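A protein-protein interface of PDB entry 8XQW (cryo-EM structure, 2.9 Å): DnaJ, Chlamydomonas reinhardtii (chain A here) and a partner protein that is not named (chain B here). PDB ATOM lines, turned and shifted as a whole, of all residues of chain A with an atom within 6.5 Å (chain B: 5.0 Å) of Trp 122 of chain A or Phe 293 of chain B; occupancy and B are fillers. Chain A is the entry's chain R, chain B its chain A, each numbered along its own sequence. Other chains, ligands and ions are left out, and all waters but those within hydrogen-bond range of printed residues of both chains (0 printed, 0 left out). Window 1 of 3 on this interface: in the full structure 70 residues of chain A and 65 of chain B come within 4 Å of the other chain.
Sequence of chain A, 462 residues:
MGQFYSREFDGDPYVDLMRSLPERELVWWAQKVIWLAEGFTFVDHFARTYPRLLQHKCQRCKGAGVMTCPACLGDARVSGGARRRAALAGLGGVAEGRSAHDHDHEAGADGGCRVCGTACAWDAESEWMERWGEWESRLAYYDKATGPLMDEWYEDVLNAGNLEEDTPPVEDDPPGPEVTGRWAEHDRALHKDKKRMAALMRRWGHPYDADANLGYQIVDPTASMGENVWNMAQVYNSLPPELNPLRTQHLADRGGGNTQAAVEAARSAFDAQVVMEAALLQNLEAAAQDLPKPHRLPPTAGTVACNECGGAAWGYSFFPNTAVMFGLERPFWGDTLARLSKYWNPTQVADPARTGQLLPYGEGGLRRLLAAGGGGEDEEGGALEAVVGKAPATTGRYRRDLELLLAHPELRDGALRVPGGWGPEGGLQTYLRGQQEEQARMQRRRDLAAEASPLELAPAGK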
ATOM      1  N   CYS A 120       1.140  28.790   4.807  1.00  0.00           N
ATOM      2  CA  CYS A 120       0.598  28.737   6.182  1.00  0.00           C
ATOM      3  C   CYS A 120       1.657  29.287   7.144  1.00  0.00           C
ATOM      4  O   CYS A 120       2.696  29.750   6.655  1.00  0.00           O
ATOM      5  CB  CYS A 120       0.222  27.312   6.536  1.00  0.00           C
ATOM      6  SG  CYS A 120      -1.354  26.775   5.833  1.00  0.00           S
ATOM      7  N   ALA A 121       1.416  29.228   8.454  1.00  0.00           N
ATOM      8  CA  ALA A 121       2.341  29.826   9.444  1.00  0.00           C
ATOM      9  C   ALA A 121       3.479  28.881   9.799  1.00  0.00           C
ATOM     10  O   ALA A 121       4.601  29.350   9.971  1.00  0.00           O
ATOM     11  CB  ALA A 121       1.548  30.129  10.665  1.00  0.00           C
ATOM     12  N   TRP A 122       3.184  27.596   9.942  1.00  0.00           N
ATOM     13  CA  TRP A 122       4.201  26.590  10.306  1.00  0.00           C
ATOM     14  C   TRP A 122       4.921  26.135   9.050  1.00  0.00           C
ATOM     15  O   TRP A 122       5.529  25.069   9.078  1.00  0.00           O
ATOM     16  CB  TRP A 122       3.527  25.415  11.014  1.00  0.00           C
ATOM     17  CG  TRP A 122       3.331  25.585  12.493  1.00  0.00           C
ATOM     18  CD1 TRP A 122       2.236  26.097  13.119  1.00  0.00           C
ATOM     19  CD2 TRP A 122       4.252  25.203  13.535  1.00  0.00           C
ATOM     20  NE1 TRP A 122       2.415  26.076  14.475  1.00  0.00           N
ATOM     21  CE2 TRP A 122       3.638  25.532  14.760  1.00  0.00           C
ATOM     22  CE3 TRP A 122       5.523  24.624  13.552  1.00  0.00           C
ATOM     23  CZ2 TRP A 122       4.256  25.300  15.984  1.00  0.00           C
ATOM     24  CZ3 TRP A 122       6.130  24.392  14.764  1.00  0.00           C
ATOM     25  CH2 TRP A 122       5.503  24.724  15.961  1.00  0.00           C
ATOM     26  N   ASP A 123       4.876  26.927   7.987  1.00  0.00           N
ATOM     27  CA  ASP A 123       5.651  26.597   6.767  1.00  0.00           C
ATOM     28  C   ASP A 123       7.025  27.245   6.876  1.00  0.00           C
ATOM     29  O   ASP A 123       7.983  26.652   6.386  1.00  0.00           O
ATOM     30  CB  ASP A 123       4.941  27.067   5.521  1.00  0.00           C
ATOM     31  CG  ASP A 123       3.582  26.439   5.279  1.00  0.00           C
ATOM     32  OD1 ASP A 123       3.151  25.648   6.132  1.00  0.00           O
ATOM     33  OD2 ASP A 123       2.974  26.754   4.242  1.00  0.00           O
ATOM     34  N   ALA A 124       7.110  28.431   7.471  1.00  0.00           N
ATOM     35  CA  ALA A 124       8.409  29.088   7.723  1.00  0.00           C
ATOM     36  C   ALA A 124       9.236  28.166   8.588  1.00  0.00           C
ATOM     37  O   ALA A 124       9.008  28.157   9.793  1.00  0.00           O
ATOM     38  CB  ALA A 124       8.132  30.349   8.455  1.00  0.00           C
ATOM     39  N   GLU A 125      10.197  27.470   8.012  1.00  0.00           N
ATOM     40  CA  GLU A 125      10.902  26.442   8.757  1.00  0.00           C
ATOM     41  C   GLU A 125      11.979  27.022   9.646  1.00  0.00           C
ATOM     42  O   GLU A 125      12.699  26.299  10.321  1.00  0.00           O
ATOM     43  CB  GLU A 125      11.516  25.433   7.802  1.00  0.00           C
ATOM     44  CG  GLU A 125      11.747  24.082   8.412  1.00  0.00           C
ATOM     45  CD  GLU A 125      12.929  23.378   7.806  1.00  0.00           C
ATOM     46  OE1 GLU A 125      13.591  22.599   8.520  1.00  0.00           O
ATOM     47  OE2 GLU A 125      13.195  23.604   6.611  1.00  0.00           O
ATOM     48  N   GLU A 127      11.313  29.295  11.955  1.00  0.00           N
ATOM     49  CA  GLU A 127      10.681  29.743  13.183  1.00  0.00           C
ATOM     50  C   GLU A 127      10.066  28.590  13.946  1.00  0.00           C
ATOM     51  O   GLU A 127       9.244  28.793  14.829  1.00  0.00           O
ATOM     52  CB  GLU A 127       9.605  30.774  12.877  1.00  0.00           C
ATOM     53  CG  GLU A 127      10.130  32.148  12.562  1.00  0.00           C
ATOM     54  CD  GLU A 127      10.728  32.241  11.179  1.00  0.00           C
ATOM     55  OE1 GLU A 127      11.307  33.296  10.845  1.00  0.00           O
ATOM     56  OE2 GLU A 127      10.627  31.254  10.426  1.00  0.00           O
ATOM     57  N   TRP A 128      10.469  27.371  13.604  1.00  0.00           N
ATOM     58  CA  TRP A 128       9.826  26.206  14.194  1.00  0.00           C
ATOM     59  C   TRP A 128      10.145  26.082  15.674  1.00  0.00           C
ATOM     60  O   TRP A 128       9.239  25.943  16.506  1.00  0.00           O
ATOM     61  CB  TRP A 128      10.252  24.948  13.446  1.00  0.00           C
ATOM     62  CG  TRP A 128       9.425  24.669  12.252  1.00  0.00           C
ATOM     63  CD1 TRP A 128       8.393  25.410  11.785  1.00  0.00           C
ATOM     64  CD2 TRP A 128       9.559  23.565  11.365  1.00  0.00           C
ATOM     65  NE1 TRP A 128       7.872  24.837  10.659  1.00  0.00           N
ATOM     66  CE2 TRP A 128       8.575  23.699  10.380  1.00  0.00           C
ATOM     67  CE3 TRP A 128      10.420  22.469  11.311  1.00  0.00           C
ATOM     68  CZ2 TRP A 128       8.423  22.786   9.360  1.00  0.00           C
ATOM     69  CZ3 TRP A 128      10.269  21.567  10.296  1.00  0.00           C
ATOM     70  CH2 TRP A 128       9.279  21.728   9.333  1.00  0.00           C
ATOM     71  N   MET A 129      11.424  26.138  16.027  1.00  0.00           N
ATOM     72  CA  MET A 129      11.808  25.865  17.402  1.00  0.00           C
ATOM     73  C   MET A 129      11.401  26.985  18.348  1.00  0.00           C
ATOM     74  O   MET A 129      11.141  26.728  19.526  1.00  0.00           O
ATOM     75  CB  MET A 129      13.305  25.600  17.462  1.00  0.00           C
ATOM     76  CG  MET A 129      13.735  24.574  16.437  1.00  0.00           C
ATOM     77  SD  MET A 129      15.121  23.562  16.960  1.00  0.00           S
ATOM     78  CE  MET A 129      16.352  24.099  15.788  1.00  0.00           C
ATOM     79  N   ARG A 131       8.505  28.774  18.041  1.00  0.00           N
ATOM     80  CA  ARG A 131       7.103  28.493  18.309  1.00  0.00           C
ATOM     81  C   ARG A 131       6.958  27.322  19.262  1.00  0.00           C
ATOM     82  O   ARG A 131       6.123  27.350  20.175  1.00  0.00           O
ATOM     83  CB  ARG A 131       6.371  28.216  17.002  1.00  0.00           C
ATOM     84  CG  ARG A 131       6.321  29.397  16.076  1.00  0.00           C
ATOM     85  CD  ARG A 131       5.812  29.007  14.710  1.00  0.00           C
ATOM     86  NE  ARG A 131       5.058  30.096  14.118  1.00  0.00           N
ATOM     87  CZ  ARG A 131       3.754  30.263  14.289  1.00  0.00           C
ATOM     88  NH1 ARG A 131       3.071  29.403  15.024  1.00  0.00           N
ATOM     89  NH2 ARG A 131       3.134  31.288  13.730  1.00  0.00           N
ATOM     90  N   TRP A 132       7.778  26.288  19.086  1.00  0.00           N
ATOM     91  CA  TRP A 132       7.674  25.173  20.014  1.00  0.00           C
ATOM     92  C   TRP A 132       8.101  25.575  21.414  1.00  0.00           C
ATOM     93  O   TRP A 132       7.527  25.090  22.393  1.00  0.00           O
ATOM     94  CB  TRP A 132       8.491  23.980  19.543  1.00  0.00           C
ATOM     95  CG  TRP A 132       8.179  22.791  20.366  1.00  0.00           C
ATOM     96  CD1 TRP A 132       9.021  22.133  21.196  1.00  0.00           C
ATOM     97  CD2 TRP A 132       6.914  22.137  20.472  1.00  0.00           C
ATOM     98  NE1 TRP A 132       8.365  21.100  21.811  1.00  0.00           N
ATOM     99  CE2 TRP A 132       7.068  21.081  21.377  1.00  0.00           C
ATOM    100  CE3 TRP A 132       5.668  22.338  19.881  1.00  0.00           C
ATOM    101  CZ2 TRP A 132       6.027  20.229  21.707  1.00  0.00           C
ATOM    102  CZ3 TRP A 132       4.638  21.491  20.207  1.00  0.00           C
ATOM    103  CH2 TRP A 132       4.821  20.452  21.110  1.00  0.00           C
ATOM    104  N   TRP A 135       5.202  27.360  23.028  1.00  0.00           N
ATOM    105  CA  TRP A 135       4.107  26.458  23.347  1.00  0.00           C
ATOM    106  C   TRP A 135       4.437  25.591  24.549  1.00  0.00           C
ATOM    107  O   TRP A 135       3.583  25.375  25.411  1.00  0.00           O
ATOM    108  CB  TRP A 135       3.749  25.604  22.135  1.00  0.00           C
ATOM    109  CG  TRP A 135       2.695  26.248  21.321  1.00  0.00           C
ATOM    110  CD1 TRP A 135       2.835  26.797  20.090  1.00  0.00           C
ATOM    111  CD2 TRP A 135       1.335  26.451  21.698  1.00  0.00           C
ATOM    112  NE1 TRP A 135       1.643  27.319  19.667  1.00  0.00           N
ATOM    113  CE2 TRP A 135       0.705  27.116  20.641  1.00  0.00           C
ATOM    114  CE3 TRP A 135       0.585  26.118  22.823  1.00  0.00           C
ATOM    115  CZ2 TRP A 135      -0.633  27.460  20.675  1.00  0.00           C
ATOM    116  CZ3 TRP A 135      -0.738  26.456  22.852  1.00  0.00           C
ATOM    117  CH2 TRP A 135      -1.337  27.122  21.789  1.00  0.00           C
ATOM    118  N   GLN A 273      -5.845  30.148  18.324  1.00  0.00           N
ATOM    119  CA  GLN A 273      -5.122  28.892  18.156  1.00  0.00           C
ATOM    120  C   GLN A 273      -5.886  27.730  18.768  1.00  0.00           C
ATOM    121  O   GLN A 273      -5.956  26.642  18.184  1.00  0.00           O
ATOM    122  CB  GLN A 273      -3.737  28.984  18.779  1.00  0.00           C
ATOM    123  CG  GLN A 273      -2.885  30.093  18.244  1.00  0.00           C
ATOM    124  CD  GLN A 273      -2.238  29.749  16.936  1.00  0.00           C
ATOM    125  OE1 GLN A 273      -2.593  30.294  15.900  1.00  0.00           O
ATOM    126  NE2 GLN A 273      -1.274  28.845  16.973  1.00  0.00           N
ATOM    127  N   LEU B 200       0.595  17.763  18.405  1.00  0.00           N
ATOM    128  CA  LEU B 200      -0.258  18.685  17.665  1.00  0.00           C
ATOM    129  C   LEU B 200      -0.912  19.615  18.671  1.00  0.00           C
ATOM    130  O   LEU B 200      -1.714  19.168  19.493  1.00  0.00           O
ATOM    131  CB  LEU B 200      -1.307  17.921  16.860  1.00  0.00           C
ATOM    132  CG  LEU B 200      -2.168  18.670  15.852  1.00  0.00           C
ATOM    133  CD1 LEU B 200      -2.517  17.754  14.710  1.00  0.00           C
ATOM    134  CD2 LEU B 200      -3.427  19.183  16.508  1.00  0.00           C
ATOM    135  N   VAL B 201      -0.594  20.903  18.606  1.00  0.00           N
ATOM    136  CA  VAL B 201      -0.912  21.839  19.674  1.00  0.00           C
ATOM    137  C   VAL B 201      -1.942  22.877  19.241  1.00  0.00           C
ATOM    138  O   VAL B 201      -2.985  23.023  19.877  1.00  0.00           O
ATOM    139  CB  VAL B 201       0.365  22.508  20.217  1.00  0.00           C
ATOM    140  CG1 VAL B 201       1.149  21.504  21.011  1.00  0.00           C
ATOM    141  CG2 VAL B 201       1.214  23.027  19.085  1.00  0.00           C
ATOM    142  N   ASP B 203      -2.984  25.605  15.599  1.00  0.00           N
ATOM    143  CA  ASP B 203      -3.205  25.546  14.160  1.00  0.00           C
ATOM    144  C   ASP B 203      -1.951  24.934  13.559  1.00  0.00           C
ATOM    145  O   ASP B 203      -0.981  25.622  13.252  1.00  0.00           O
ATOM    146  CB  ASP B 203      -3.491  26.934  13.613  1.00  0.00           C
ATOM    147  CG  ASP B 203      -3.350  27.015  12.113  1.00  0.00           C
ATOM    148  OD1 ASP B 203      -4.340  26.738  11.409  1.00  0.00           O
ATOM    149  OD2 ASP B 203      -2.257  27.375  11.632  1.00  0.00           O
ATOM    150  N   MET B 204      -1.953  23.609  13.415  1.00  0.00           N
ATOM    151  CA  MET B 204      -0.763  22.863  13.031  1.00  0.00           C
ATOM    152  C   MET B 204      -0.737  22.507  11.554  1.00  0.00           C
ATOM    153  O   MET B 204       0.022  21.628  11.154  1.00  0.00           O
ATOM    154  CB  MET B 204      -0.646  21.594  13.865  1.00  0.00           C
ATOM    155  CG  MET B 204       0.158  21.742  15.134  1.00  0.00           C
ATOM    156  SD  MET B 204       1.828  22.308  14.849  1.00  0.00           S
ATOM    157  CE  MET B 204       2.747  21.102  15.770  1.00  0.00           C
ATOM    158  N   ARG B 205      -1.534  23.171  10.732  1.00  0.00           N
ATOM    159  CA  ARG B 205      -1.551  22.872   9.313  1.00  0.00           C
ATOM    160  C   ARG B 205      -0.246  23.268   8.649  1.00  0.00           C
ATOM    161  O   ARG B 205       0.433  24.198   9.076  1.00  0.00           O
ATOM    162  CB  ARG B 205      -2.678  23.615   8.620  1.00  0.00           C
ATOM    163  CG  ARG B 205      -4.014  23.411   9.216  1.00  0.00           C
ATOM    164  CD  ARG B 205      -4.979  24.349   8.562  1.00  0.00           C
ATOM    165  NE  ARG B 205      -4.766  25.714   9.011  1.00  0.00           N
ATOM    166  CZ  ARG B 205      -5.358  26.775   8.481  1.00  0.00           C
ATOM    167  NH1 ARG B 205      -6.197  26.629   7.469  1.00  0.00           N
ATOM    168  NH2 ARG B 205      -5.104  27.983   8.961  1.00  0.00           N
ATOM    169  N   ILE B 206       0.097  22.548   7.588  1.00  0.00           N
ATOM    170  CA  ILE B 206       1.096  22.988   6.631  1.00  0.00           C
ATOM    171  C   ILE B 206       0.454  22.962   5.257  1.00  0.00           C
ATOM    172  O   ILE B 206      -0.566  22.320   5.037  1.00  0.00           O
ATOM    173  CB  ILE B 206       2.368  22.134   6.652  1.00  0.00           C
ATOM    174  CG1 ILE B 206       2.018  20.663   6.729  1.00  0.00           C
ATOM    175  CG2 ILE B 206       3.232  22.508   7.801  1.00  0.00           C
ATOM    176  CD1 ILE B 206       3.190  19.780   6.485  1.00  0.00           C
ATOM    177  N   ALA B 232      -3.885  13.701   5.798  1.00  0.00           N
ATOM    178  CA  ALA B 232      -2.716  13.028   6.328  1.00  0.00           C
ATOM    179  C   ALA B 232      -2.225  13.761   7.559  1.00  0.00           C
ATOM    180  O   ALA B 232      -2.463  14.959   7.727  1.00  0.00           O
ATOM    181  CB  ALA B 232      -1.609  12.940   5.287  1.00  0.00           C
ATOM    182  N   VAL B 233      -1.559  13.020   8.431  1.00  0.00           N
ATOM    183  CA  VAL B 233      -0.867  13.574   9.584  1.00  0.00           C
ATOM    184  C   VAL B 233       0.610  13.293   9.393  1.00  0.00           C
ATOM    185  O   VAL B 233       1.061  12.160   9.574  1.00  0.00           O
ATOM    186  CB  VAL B 233      -1.378  12.976  10.897  1.00  0.00           C
ATOM    187  CG1 VAL B 233      -0.456  13.324  12.014  1.00  0.00           C
ATOM    188  CG2 VAL B 233      -2.742  13.494  11.189  1.00  0.00           C
ATOM    189  N   VAL B 234       1.357  14.317   9.028  1.00  0.00           N
ATOM    190  CA  VAL B 234       2.773  14.200   8.719  1.00  0.00           C
ATOM    191  C   VAL B 234       3.563  14.367  10.003  1.00  0.00           C
ATOM    192  O   VAL B 234       3.363  15.336  10.735  1.00  0.00           O
ATOM    193  CB  VAL B 234       3.190  15.252   7.685  1.00  0.00           C
ATOM    194  CG1 VAL B 234       4.495  14.897   7.089  1.00  0.00           C
ATOM    195  CG2 VAL B 234       2.154  15.357   6.625  1.00  0.00           C
ATOM    196  N   VAL B 236       7.239  14.903  11.575  1.00  0.00           N
ATOM    197  CA  VAL B 236       8.569  15.381  11.226  1.00  0.00           C
ATOM    198  C   VAL B 236       9.375  15.506  12.509  1.00  0.00           C
ATOM    199  O   VAL B 236       8.939  16.176  13.443  1.00  0.00           O
ATOM    200  CB  VAL B 236       8.523  16.728  10.488  1.00  0.00           C
ATOM    201  CG1 VAL B 236       9.812  16.977   9.784  1.00  0.00           C
ATOM    202  CG2 VAL B 236       7.401  16.750   9.508  1.00  0.00           C
ATOM    203  N   TYR B 291       7.091  16.812  15.567  1.00  0.00           N
ATOM    204  CA  TYR B 291       5.907  17.576  15.220  1.00  0.00           C
ATOM    205  C   TYR B 291       4.937  16.700  14.450  1.00  0.00           C
ATOM    206  O   TYR B 291       5.339  15.866  13.636  1.00  0.00           O
ATOM    207  CB  TYR B 291       6.253  18.770  14.345  1.00  0.00           C
ATOM    208  CG  TYR B 291       7.398  19.622  14.794  1.00  0.00           C
ATOM    209  CD1 TYR B 291       7.327  20.354  15.959  1.00  0.00           C
ATOM    210  CD2 TYR B 291       8.534  19.735  14.022  1.00  0.00           C
ATOM    211  CE1 TYR B 291       8.361  21.144  16.352  1.00  0.00           C
ATOM    212  CE2 TYR B 291       9.570  20.521  14.411  1.00  0.00           C
ATOM    213  CZ  TYR B 291       9.478  21.226  15.573  1.00  0.00           C
ATOM    214  OH  TYR B 291      10.519  22.016  15.968  1.00  0.00           O
ATOM    215  N   ARG B 292       3.647  16.925  14.671  1.00  0.00           N
ATOM    216  CA  ARG B 292       2.600  16.195  13.974  1.00  0.00           C
ATOM    217  C   ARG B 292       1.694  17.183  13.260  1.00  0.00           C
ATOM    218  O   ARG B 292       0.687  17.613  13.819  1.00  0.00           O
ATOM    219  CB  ARG B 292       1.800  15.335  14.940  1.00  0.00           C
ATOM    220  CG  ARG B 292       2.470  14.033  15.251  1.00  0.00           C
ATOM    221  CD  ARG B 292       1.834  13.345  16.421  1.00  0.00           C
ATOM    222  NE  ARG B 292       2.841  12.994  17.409  1.00  0.00           N
ATOM    223  CZ  ARG B 292       3.367  11.787  17.529  1.00  0.00           C
ATOM    224  NH1 ARG B 292       2.972  10.816  16.730  1.00  0.00           N
ATOM    225  NH2 ARG B 292       4.287  11.552  18.446  1.00  0.00           N
ATOM    226  N   PHE B 293       2.027  17.511  12.019  1.00  0.00           N
ATOM    227  CA  PHE B 293       1.277  18.466  11.223  1.00  0.00           C
ATOM    228  C   PHE B 293       0.099  17.796  10.543  1.00  0.00           C
ATOM    229  O   PHE B 293       0.102  16.593  10.305  1.00  0.00           O
ATOM    230  CB  PHE B 293       2.161  19.096  10.161  1.00  0.00           C
ATOM    231  CG  PHE B 293       3.341  19.812  10.705  1.00  0.00           C
ATOM    232  CD1 PHE B 293       3.187  20.936  11.466  1.00  0.00           C
ATOM    233  CD2 PHE B 293       4.610  19.364  10.446  1.00  0.00           C
ATOM    234  CE1 PHE B 293       4.266  21.589  11.950  1.00  0.00           C
ATOM    235  CE2 PHE B 293       5.687  20.019  10.938  1.00  0.00           C
ATOM    236  CZ  PHE B 293       5.514  21.129  11.690  1.00  0.00           C
ATOM    237  N   TYR B 294      -0.889  18.600  10.196  1.00  0.00           N
ATOM    238  CA  TYR B 294      -2.090  18.143   9.523  1.00  0.00           C
ATOM    239  C   TYR B 294      -2.077  18.688   8.106  1.00  0.00           C
ATOM    240  O   TYR B 294      -1.778  19.862   7.904  1.00  0.00           O
ATOM    241  CB  TYR B 294      -3.305  18.639  10.301  1.00  0.00           C
ATOM    242  CG  TYR B 294      -4.626  18.661   9.589  1.00  0.00           C
ATOM    243  CD1 TYR B 294      -4.930  19.634   8.669  1.00  0.00           C
ATOM    244  CD2 TYR B 294      -5.600  17.743   9.895  1.00  0.00           C
ATOM    245  CE1 TYR B 294      -6.137  19.658   8.044  1.00  0.00           C
ATOM    246  CE2 TYR B 294      -6.811  17.770   9.278  1.00  0.00           C
ATOM    247  CZ  TYR B 294      -7.069  18.725   8.356  1.00  0.00           C
ATOM    248  OH  TYR B 294      -8.284  18.746   7.736  1.00  0.00           O
ATOM    249  N   VAL B 295      -2.397  17.856   7.121  1.00  0.00           N
ATOM    250  CA  VAL B 295      -2.370  18.317   5.740  1.00  0.00           C
ATOM    251  C   VAL B 295      -3.569  17.759   4.991  1.00  0.00           C
ATOM    252  O   VAL B 295      -3.981  16.616   5.212  1.00  0.00           O
ATOM    253  CB  VAL B 295      -1.049  17.938   5.053  1.00  0.00           C
ATOM    254  CG1 VAL B 295      -0.868  16.479   5.078  1.00  0.00           C
ATOM    255  CG2 VAL B 295      -1.024  18.431   3.650  1.00  0.00           C
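The side-chain carboxylate (OD1) of Asp 203 of chain B is in salt-bridge range of the guanidinium group (NE) of Arg 205 of chain B.
O of Tyr 294 of chain B lies within hydrogen-bond range of N of Ile 206 of chain B.
The backbone NH (N) of Tyr 294 of chain B sits at hydrogen-bond distance from the backbone carbonyl oxygen (O) of Met 204 of chain B.
The backbone NH (N) of Cys 120 of chain A sits at hydrogen-bond distance from the side-chain carboxylate (OD2) of Asp 123 of chain A, at 2.8 Å.
The backbone NH (N) of Phe 293 of chain B lies within hydrogen-bond range of the backbone carbonyl oxygen (O) of Val 234 of chain B (2.9 Å).
O of Val 236 of chain B lies within hydrogen-bond range of N of Tyr 291 of chain B (2.9 Å).
Trp 122 of chain A touches Asp 203 of chain B.
Trp 122 of chain A touches Met 204 of chain B.
Trp 122 of chain A touches Arg 205 of chain B.
Trp 122 of chain A touches Ile 206 of chain B.
Trp 122 of chain A touches Phe 293 of chain B (CE3 to CE1, 3.7 Å).
Ile 206 of chain B touches Asp 123 of chain A (CA to OD1, 3.4 Å).
Tyr 291 of chain B touches Trp 128 of chain A.
CZ3 of Trp 132 of chain A touches CG1 of Val 201 of chain B, 3.6 Å away.
Gln 273 of chain A touches Asp 203 of chain B.
Of the printed residues of chain B, Trp 128 of chain A touches Tyr 291 (3.8 Å).
Leu 200 of chain B touches none of the printed residues of chain A.
Of the printed residues of chain A, Val 201 of chain B touches Trp 132 (3.6 Å).
Phe 293 of chain B touches just one residue of chain A: Trp 122.
The nearest residue of chain B that does not touch Trp 122 of chain A is Tyr 291 of chain B (4.2 Å).
The nearest residue of chain A that does not touch Phe 293 of chain B is Trp 128 of chain A (4.1 Å).
Hydrophobic or aromatic side chains of chain A that line the printed part of chain B: Trp 122, Trp 128 and Trp 132.
Along chain A the printed residues that touch a printed residue of chain B span positions 122 to 273.
Of the 15 printed residues of chain B, 7 touch a printed residue of chain A.
Along chain B the printed residues that touch a printed residue of chain A span positions 201 to 293.
Among the printed residues, 9 pairs touch across the chains.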
